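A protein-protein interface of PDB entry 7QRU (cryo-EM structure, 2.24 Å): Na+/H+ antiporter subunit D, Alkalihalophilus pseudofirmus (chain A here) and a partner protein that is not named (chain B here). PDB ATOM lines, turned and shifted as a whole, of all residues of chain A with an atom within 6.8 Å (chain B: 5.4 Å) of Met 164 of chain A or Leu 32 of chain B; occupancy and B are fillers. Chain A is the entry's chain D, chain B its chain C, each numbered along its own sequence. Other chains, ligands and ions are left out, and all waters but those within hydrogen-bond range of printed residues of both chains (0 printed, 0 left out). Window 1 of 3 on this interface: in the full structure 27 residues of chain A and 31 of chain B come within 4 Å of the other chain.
O of Leu 32 of chain B sits at hydrogen-bond distance from OG of Ser 36 of chain B.
Printed residues of chain A that touch a printed residue of chain B: Leu 160, Met 164, Phe 168 and Ile 171. Hydrophobic or aromatic side chains of chain B within 4 Å of the printed part of chain A: Ile 20, Leu 25, Val 28, Val 29, Leu 32, Leu 35 and Leu 87. Among the printed residues, 10 pairs touch across the chains.
Of the printed residues of chain B, Met 164 of chain A touches Val 28, Val 29 and Leu 32. Of the printed residues of chain B, Phe 168 of chain A touches Ile 20 and Leu 35. Printed residues of chain A within 4 Å of Leu 25 of chain B: Leu 160 (3.5 Å). Of the printed residues of chain A, Val 29 of chain B touches Met 164. Printed residues of chain A within 4 Å of Leu 35 of chain B: Phe 168 and Ile 171. Printed residues of chain A within 4 Å of Leu 87 of chain B: Leu 160 (3.6 Å). The nearest printed residue of chain B that does not touch Met 164 of chain A is Leu 25 of chain B (4.01 Å). The nearest residue of chain A that does not touch Leu 32 of chain B is Val 167 of chain A (4.1 Å). The nearest printed residue of chain A that does not touch Ile 20 of chain B is Met 164 of chain A (6.9 Å).
Among the printed residues, pairs that only touch across the chains: Leu 160 of chain A with Leu 25 of chain B (3.5 Å), Met 164 of chain A with Val 28 of chain B (3.5 Å), Leu 160 of chain A with Leu 87 of chain B (3.6 Å), Ile 171 of chain A with Ser 36 of chain B (3.7 Å), Met 164 of chain A with Val 29 of chain B (3.8 Å), Phe 168 of chain A with Ile 20 of chain B (3.8 Å), Met 164 of chain A with Leu 32 of chain B (3.8 Å), Ile 171 of chain A with Leu 35 of chain B (3.8 Å), Phe 168 of chain A with Leu 35 of chain B (3.9 Å) and Ile 171 of chain A with Leu 32 of chain B (3.9 Å).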
ATOM      1  N   TYR A 144      10.829  17.115  29.195  1.00  0.00           N
ATOM      2  CA  TYR A 144       9.469  17.087  28.688  1.00  0.00           C
ATOM      3  C   TYR A 144       8.575  17.912  29.606  1.00  0.00           C
ATOM      4  O   TYR A 144       7.706  18.626  29.122  1.00  0.00           O
ATOM      5  CB  TYR A 144       8.834  15.695  28.594  1.00  0.00           C
ATOM      6  CG  TYR A 144       9.541  14.781  27.636  1.00  0.00           C
ATOM      7  CD1 TYR A 144      10.390  15.254  26.627  1.00  0.00           C
ATOM      8  CD2 TYR A 144       9.277  13.439  27.676  1.00  0.00           C
ATOM      9  CE1 TYR A 144      11.084  14.388  25.819  1.00  0.00           C
ATOM     10  CE2 TYR A 144       9.941  12.542  26.848  1.00  0.00           C
ATOM     11  CZ  TYR A 144      10.857  13.005  25.928  1.00  0.00           C
ATOM     12  OH  TYR A 144      11.384  11.989  25.112  1.00  0.00           O
ATOM     13  N   SER A 159       5.575  21.567  22.531  1.00  0.00           N
ATOM     14  CA  SER A 159       6.007  20.547  23.462  1.00  0.00           C
ATOM     15  C   SER A 159       5.525  19.180  23.015  1.00  0.00           C
ATOM     16  O   SER A 159       6.350  18.271  22.824  1.00  0.00           O
ATOM     17  CB  SER A 159       5.540  20.870  24.850  1.00  0.00           C
ATOM     18  OG  SER A 159       6.046  22.164  25.171  1.00  0.00           O
ATOM     19  N   LEU A 160       4.307  19.131  22.502  1.00  0.00           N
ATOM     20  CA  LEU A 160       3.805  17.891  21.975  1.00  0.00           C
ATOM     21  C   LEU A 160       4.659  17.374  20.830  1.00  0.00           C
ATOM     22  O   LEU A 160       5.044  16.237  20.906  1.00  0.00           O
ATOM     23  CB  LEU A 160       2.371  17.992  21.506  1.00  0.00           C
ATOM     24  CG  LEU A 160       1.818  16.680  20.962  1.00  0.00           C
ATOM     25  CD1 LEU A 160       1.911  15.516  21.999  1.00  0.00           C
ATOM     26  CD2 LEU A 160       0.392  16.909  20.608  1.00  0.00           C
ATOM     27  N   LYS A 161       5.098  18.223  19.885  1.00  0.00           N
ATOM     28  CA  LYS A 161       5.996  17.730  18.863  1.00  0.00           C
ATOM     29  C   LYS A 161       7.377  17.340  19.404  1.00  0.00           C
ATOM     30  O   LYS A 161       7.911  16.281  19.070  1.00  0.00           O
ATOM     31  CB  LYS A 161       6.090  18.767  17.764  1.00  0.00           C
ATOM     32  CG  LYS A 161       4.768  19.118  17.070  1.00  0.00           C
ATOM     33  CD  LYS A 161       4.853  20.318  16.174  1.00  0.00           C
ATOM     34  CE  LYS A 161       3.538  21.029  15.948  1.00  0.00           C
ATOM     35  NZ  LYS A 161       3.732  22.367  15.309  1.00  0.00           N
ATOM     36  N   TYR A 162       7.943  18.124  20.331  1.00  0.00           N
ATOM     37  CA  TYR A 162       9.212  17.813  20.967  1.00  0.00           C
ATOM     38  C   TYR A 162       9.094  16.439  21.617  1.00  0.00           C
ATOM     39  O   TYR A 162       9.967  15.628  21.558  1.00  0.00           O
ATOM     40  CB  TYR A 162       9.532  18.953  21.940  1.00  0.00           C
ATOM     41  CG  TYR A 162      10.671  18.707  22.846  1.00  0.00           C
ATOM     42  CD1 TYR A 162      11.981  18.973  22.476  1.00  0.00           C
ATOM     43  CD2 TYR A 162      10.428  18.279  24.129  1.00  0.00           C
ATOM     44  CE1 TYR A 162      13.027  18.777  23.321  1.00  0.00           C
ATOM     45  CE2 TYR A 162      11.508  18.021  24.965  1.00  0.00           C
ATOM     46  CZ  TYR A 162      12.804  18.253  24.579  1.00  0.00           C
ATOM     47  OH  TYR A 162      13.883  18.088  25.428  1.00  0.00           O
ATOM     48  N   VAL A 163       8.066  16.178  22.408  1.00  0.00           N
ATOM     49  CA  VAL A 163       8.042  14.884  23.065  1.00  0.00           C
ATOM     50  C   VAL A 163       7.928  13.795  22.000  1.00  0.00           C
ATOM     51  O   VAL A 163       8.709  12.884  22.117  1.00  0.00           O
ATOM     52  CB  VAL A 163       6.887  14.831  24.051  1.00  0.00           C
ATOM     53  CG1 VAL A 163       6.774  13.439  24.614  1.00  0.00           C
ATOM     54  CG2 VAL A 163       7.077  15.857  25.128  1.00  0.00           C
ATOM     55  N   MET A 164       7.042  13.872  20.956  1.00  0.00           N
ATOM     56  CA  MET A 164       6.903  12.754  19.985  1.00  0.00           C
ATOM     57  C   MET A 164       8.177  12.428  19.253  1.00  0.00           C
ATOM     58  O   MET A 164       8.604  11.276  19.165  1.00  0.00           O
ATOM     59  CB  MET A 164       5.797  12.991  18.950  1.00  0.00           C
ATOM     60  CG  MET A 164       4.467  12.730  19.709  1.00  0.00           C
ATOM     61  SD  MET A 164       3.125  13.521  18.992  1.00  0.00           S
ATOM     62  CE  MET A 164       1.720  12.558  19.522  1.00  0.00           C
ATOM     63  N   ILE A 165       8.874  13.463  18.827  1.00  0.00           N
ATOM     64  CA  ILE A 165      10.140  13.219  18.157  1.00  0.00           C
ATOM     65  C   ILE A 165      11.152  12.594  19.080  1.00  0.00           C
ATOM     66  O   ILE A 165      11.876  11.709  18.616  1.00  0.00           O
ATOM     67  CB  ILE A 165      10.664  14.479  17.467  1.00  0.00           C
ATOM     68  CG1 ILE A 165       9.745  14.802  16.305  1.00  0.00           C
ATOM     69  CG2 ILE A 165      12.031  14.285  16.964  1.00  0.00           C
ATOM     70  CD1 ILE A 165       9.754  16.265  15.953  1.00  0.00           C
ATOM     71  N   ASN A 166      11.265  13.082  20.327  1.00  0.00           N
ATOM     72  CA  ASN A 166      12.223  12.511  21.255  1.00  0.00           C
ATOM     73  C   ASN A 166      11.860  11.079  21.619  1.00  0.00           C
ATOM     74  O   ASN A 166      12.771  10.244  21.737  1.00  0.00           O
ATOM     75  CB  ASN A 166      12.458  13.366  22.492  1.00  0.00           C
ATOM     76  CG  ASN A 166      13.460  14.460  22.182  1.00  0.00           C
ATOM     77  OD1 ASN A 166      14.618  14.073  22.061  1.00  0.00           O
ATOM     78  ND2 ASN A 166      13.031  15.725  21.902  1.00  0.00           N
ATOM     79  N   VAL A 167      10.595  10.750  21.761  1.00  0.00           N
ATOM     80  CA  VAL A 167      10.246   9.363  22.007  1.00  0.00           C
ATOM     81  C   VAL A 167      10.734   8.498  20.847  1.00  0.00           C
ATOM     82  O   VAL A 167      11.362   7.467  21.074  1.00  0.00           O
ATOM     83  CB  VAL A 167       8.747   9.223  22.229  1.00  0.00           C
ATOM     84  CG1 VAL A 167       8.285   7.783  22.173  1.00  0.00           C
ATOM     85  CG2 VAL A 167       8.427   9.906  23.514  1.00  0.00           C
ATOM     86  N   PHE A 168      10.517   8.933  19.609  1.00  0.00           N
ATOM     87  CA  PHE A 168      11.020   8.166  18.484  1.00  0.00           C
ATOM     88  C   PHE A 168      12.526   7.952  18.480  1.00  0.00           C
ATOM     89  O   PHE A 168      13.003   6.823  18.234  1.00  0.00           O
ATOM     90  CB  PHE A 168      10.576   8.841  17.217  1.00  0.00           C
ATOM     91  CG  PHE A 168      11.036   8.165  15.977  1.00  0.00           C
ATOM     92  CD1 PHE A 168      10.261   7.136  15.441  1.00  0.00           C
ATOM     93  CD2 PHE A 168      12.167   8.610  15.295  1.00  0.00           C
ATOM     94  CE1 PHE A 168      10.595   6.559  14.215  1.00  0.00           C
ATOM     95  CE2 PHE A 168      12.513   7.985  14.090  1.00  0.00           C
ATOM     96  CZ  PHE A 168      11.713   6.986  13.547  1.00  0.00           C
ATOM     97  N   ALA A 169      13.312   9.006  18.784  1.00  0.00           N
ATOM     98  CA  ALA A 169      14.761   8.842  18.869  1.00  0.00           C
ATOM     99  C   ALA A 169      15.133   7.837  19.985  1.00  0.00           C
ATOM    100  O   ALA A 169      16.052   7.097  19.814  1.00  0.00           O
ATOM    101  CB  ALA A 169      15.447  10.165  19.163  1.00  0.00           C
ATOM    102  N   ILE A 171      13.425   5.186  20.890  1.00  0.00           N
ATOM    103  CA  ILE A 171      13.227   3.868  20.330  1.00  0.00           C
ATOM    104  C   ILE A 171      14.379   3.469  19.439  1.00  0.00           C
ATOM    105  O   ILE A 171      14.797   2.317  19.480  1.00  0.00           O
ATOM    106  CB  ILE A 171      11.883   3.856  19.580  1.00  0.00           C
ATOM    107  CG1 ILE A 171      10.744   3.948  20.574  1.00  0.00           C
ATOM    108  CG2 ILE A 171      11.711   2.644  18.733  1.00  0.00           C
ATOM    109  CD1 ILE A 171       9.464   4.503  20.017  1.00  0.00           C
ATOM    110  N   GLY B  16       4.016   0.945  12.646  1.00  0.00           N
ATOM    111  CA  GLY B  16       4.178   1.971  13.650  1.00  0.00           C
ATOM    112  C   GLY B  16       4.666   3.231  12.908  1.00  0.00           C
ATOM    113  O   GLY B  16       4.159   4.301  13.118  1.00  0.00           O
ATOM    114  N   ILE B  20       2.720   7.025  12.636  1.00  0.00           N
ATOM    115  CA  ILE B  20       3.195   8.294  13.127  1.00  0.00           C
ATOM    116  C   ILE B  20       3.184   9.324  11.983  1.00  0.00           C
ATOM    117  O   ILE B  20       3.268  10.543  12.286  1.00  0.00           O
ATOM    118  CB  ILE B  20       4.579   8.227  13.803  1.00  0.00           C
ATOM    119  CG1 ILE B  20       5.650   7.917  12.777  1.00  0.00           C
ATOM    120  CG2 ILE B  20       4.685   7.236  14.956  1.00  0.00           C
ATOM    121  CD1 ILE B  20       7.063   7.797  13.424  1.00  0.00           C
ATOM    122  N   LEU B  25      -3.759  12.706  16.219  1.00  0.00           N
ATOM    123  CA  LEU B  25      -3.042  12.656  17.492  1.00  0.00           C
ATOM    124  C   LEU B  25      -3.033  11.267  18.089  1.00  0.00           C
ATOM    125  O   LEU B  25      -1.957  10.819  18.525  1.00  0.00           O
ATOM    126  CB  LEU B  25      -3.718  13.624  18.480  1.00  0.00           C
ATOM    127  CG  LEU B  25      -2.799  14.433  19.343  1.00  0.00           C
ATOM    128  CD1 LEU B  25      -1.517  14.746  18.614  1.00  0.00           C
ATOM    129  CD2 LEU B  25      -3.452  15.751  19.753  1.00  0.00           C
ATOM    130  N   ARG B  27      -3.655   8.358  16.585  1.00  0.00           N
ATOM    131  CA  ARG B  27      -2.909   7.431  15.765  1.00  0.00           C
ATOM    132  C   ARG B  27      -1.414   7.597  15.913  1.00  0.00           C
ATOM    133  O   ARG B  27      -0.709   6.617  15.885  1.00  0.00           O
ATOM    134  CB  ARG B  27      -3.288   7.531  14.317  1.00  0.00           C
ATOM    135  CG  ARG B  27      -4.659   6.931  14.067  1.00  0.00           C
ATOM    136  CD  ARG B  27      -4.840   6.940  12.578  1.00  0.00           C
ATOM    137  NE  ARG B  27      -5.991   6.219  12.056  1.00  0.00           N
ATOM    138  CZ  ARG B  27      -7.203   6.735  11.961  1.00  0.00           C
ATOM    139  NH1 ARG B  27      -7.402   8.050  11.916  1.00  0.00           N
ATOM    140  NH2 ARG B  27      -8.226   5.908  11.864  1.00  0.00           N
ATOM    141  N   VAL B  28      -0.921   8.779  16.187  1.00  0.00           N
ATOM    142  CA  VAL B  28       0.507   8.938  16.392  1.00  0.00           C
ATOM    143  C   VAL B  28       0.932   8.270  17.701  1.00  0.00           C
ATOM    144  O   VAL B  28       1.976   7.587  17.791  1.00  0.00           O
ATOM    145  CB  VAL B  28       0.890  10.439  16.291  1.00  0.00           C
ATOM    146  CG1 VAL B  28       2.342  10.694  16.605  1.00  0.00           C
ATOM    147  CG2 VAL B  28       0.579  10.860  14.871  1.00  0.00           C
ATOM    148  N   VAL B  29       0.171   8.496  18.743  1.00  0.00           N
ATOM    149  CA  VAL B  29       0.513   7.843  19.995  1.00  0.00           C
ATOM    150  C   VAL B  29       0.484   6.297  19.838  1.00  0.00           C
ATOM    151  O   VAL B  29       1.417   5.608  20.241  1.00  0.00           O
ATOM    152  CB  VAL B  29      -0.417   8.366  21.081  1.00  0.00           C
ATOM    153  CG1 VAL B  29      -0.194   7.594  22.380  1.00  0.00           C
ATOM    154  CG2 VAL B  29      -0.159   9.836  21.321  1.00  0.00           C
ATOM    155  N   VAL B  30      -0.524   5.731  19.158  1.00  0.00           N
ATOM    156  CA  VAL B  30      -0.482   4.316  18.933  1.00  0.00           C
ATOM    157  C   VAL B  30       0.726   3.859  18.111  1.00  0.00           C
ATOM    158  O   VAL B  30       1.384   2.892  18.463  1.00  0.00           O
ATOM    159  CB  VAL B  30      -1.794   3.859  18.290  1.00  0.00           C
ATOM    160  CG1 VAL B  30      -1.698   2.435  17.929  1.00  0.00           C
ATOM    161  CG2 VAL B  30      -2.904   4.002  19.269  1.00  0.00           C
ATOM    162  N   GLY B  31       1.087   4.553  17.033  1.00  0.00           N
ATOM    163  CA  GLY B  31       2.262   4.211  16.281  1.00  0.00           C
ATOM    164  C   GLY B  31       3.492   4.144  17.189  1.00  0.00           C
ATOM    165  O   GLY B  31       4.265   3.162  17.063  1.00  0.00           O
ATOM    166  N   LEU B  32       3.583   5.115  18.153  1.00  0.00           N
ATOM    167  CA  LEU B  32       4.738   5.165  19.034  1.00  0.00           C
ATOM    168  C   LEU B  32       4.717   3.987  19.995  1.00  0.00           C
ATOM    169  O   LEU B  32       5.759   3.342  20.104  1.00  0.00           O
ATOM    170  CB  LEU B  32       4.806   6.501  19.779  1.00  0.00           C
ATOM    171  CG  LEU B  32       5.291   7.676  18.911  1.00  0.00           C
ATOM    172  CD1 LEU B  32       5.150   8.957  19.701  1.00  0.00           C
ATOM    173  CD2 LEU B  32       6.713   7.447  18.430  1.00  0.00           C
ATOM    174  N   ILE B  33       3.533   3.555  20.460  1.00  0.00           N
ATOM    175  CA  ILE B  33       3.411   2.307  21.222  1.00  0.00           C
ATOM    176  C   ILE B  33       3.766   1.071  20.395  1.00  0.00           C
ATOM    177  O   ILE B  33       4.542   0.247  20.859  1.00  0.00           O
ATOM    178  CB  ILE B  33       1.996   2.204  21.759  1.00  0.00           C
ATOM    179  CG1 ILE B  33       1.763   3.197  22.872  1.00  0.00           C
ATOM    180  CG2 ILE B  33       1.646   0.795  22.168  1.00  0.00           C
ATOM    181  CD1 ILE B  33       0.219   3.343  23.155  1.00  0.00           C
ATOM    182  N   LEU B  34       3.351   0.978  19.127  1.00  0.00           N
ATOM    183  CA  LEU B  34       3.842  -0.162  18.402  1.00  0.00           C
ATOM    184  C   LEU B  34       5.367  -0.172  18.176  1.00  0.00           C
ATOM    185  O   LEU B  34       5.983  -1.248  18.123  1.00  0.00           O
ATOM    186  CB  LEU B  34       3.113  -0.171  17.057  1.00  0.00           C
ATOM    187  CG  LEU B  34       1.618  -0.404  17.053  1.00  0.00           C
ATOM    188  CD1 LEU B  34       1.174  -0.516  15.593  1.00  0.00           C
ATOM    189  CD2 LEU B  34       1.265  -1.667  17.750  1.00  0.00           C
ATOM    190  N   LEU B  35       5.989   0.983  17.888  1.00  0.00           N
ATOM    191  CA  LEU B  35       7.416   0.970  17.703  1.00  0.00           C
ATOM    192  C   LEU B  35       8.087   0.514  19.002  1.00  0.00           C
ATOM    193  O   LEU B  35       9.093  -0.231  18.911  1.00  0.00           O
ATOM    194  CB  LEU B  35       7.923   2.333  17.238  1.00  0.00           C
ATOM    195  CG  LEU B  35       7.351   2.787  15.898  1.00  0.00           C
ATOM    196  CD1 LEU B  35       7.734   4.195  15.560  1.00  0.00           C
ATOM    197  CD2 LEU B  35       7.856   1.900  14.803  1.00  0.00           C
ATOM    198  N   SER B  36       7.595   0.940  20.153  1.00  0.00           N
ATOM    199  CA  SER B  36       8.232   0.446  21.364  1.00  0.00           C
ATOM    200  C   SER B  36       8.119  -1.075  21.414  1.00  0.00           C
ATOM    201  O   SER B  36       9.140  -1.705  21.691  1.00  0.00           O
ATOM    202  CB  SER B  36       7.684   1.061  22.612  1.00  0.00           C
ATOM    203  OG  SER B  36       7.523   2.479  22.446  1.00  0.00           O
ATOM    204  N   HIS B  37       6.911  -1.662  21.164  1.00  0.00           N
ATOM    205  CA  HIS B  37       6.784  -3.120  21.187  1.00  0.00           C
ATOM    206  C   HIS B  37       7.782  -3.752  20.263  1.00  0.00           C
ATOM    207  O   HIS B  37       8.475  -4.690  20.628  1.00  0.00           O
ATOM    208  CB  HIS B  37       5.424  -3.628  20.780  1.00  0.00           C
ATOM    209  CG  HIS B  37       4.378  -3.332  21.783  1.00  0.00           C
ATOM    210  ND1 HIS B  37       4.636  -3.248  23.096  1.00  0.00           N
ATOM    211  CD2 HIS B  37       3.045  -3.127  21.586  1.00  0.00           C
ATOM    212  CE1 HIS B  37       3.476  -3.112  23.722  1.00  0.00           C
ATOM    213  NE2 HIS B  37       2.493  -2.955  22.814  1.00  0.00           N
ATOM    214  N   LEU B  87       2.934  11.330  27.730  1.00  0.00           N
ATOM    215  CA  LEU B  87       2.470  11.695  26.394  1.00  0.00           C
ATOM    216  C   LEU B  87       0.957  11.639  26.192  1.00  0.00           C
ATOM    217  O   LEU B  87       0.449  12.500  25.573  1.00  0.00           O
ATOM    218  CB  LEU B  87       3.199  10.797  25.413  1.00  0.00           C
ATOM    219  CG  LEU B  87       2.826  10.938  23.959  1.00  0.00           C
ATOM    220  CD1 LEU B  87       2.981  12.376  23.436  1.00  0.00           C
ATOM    221  CD2 LEU B  87       3.720  10.022  23.227  1.00  0.00           C
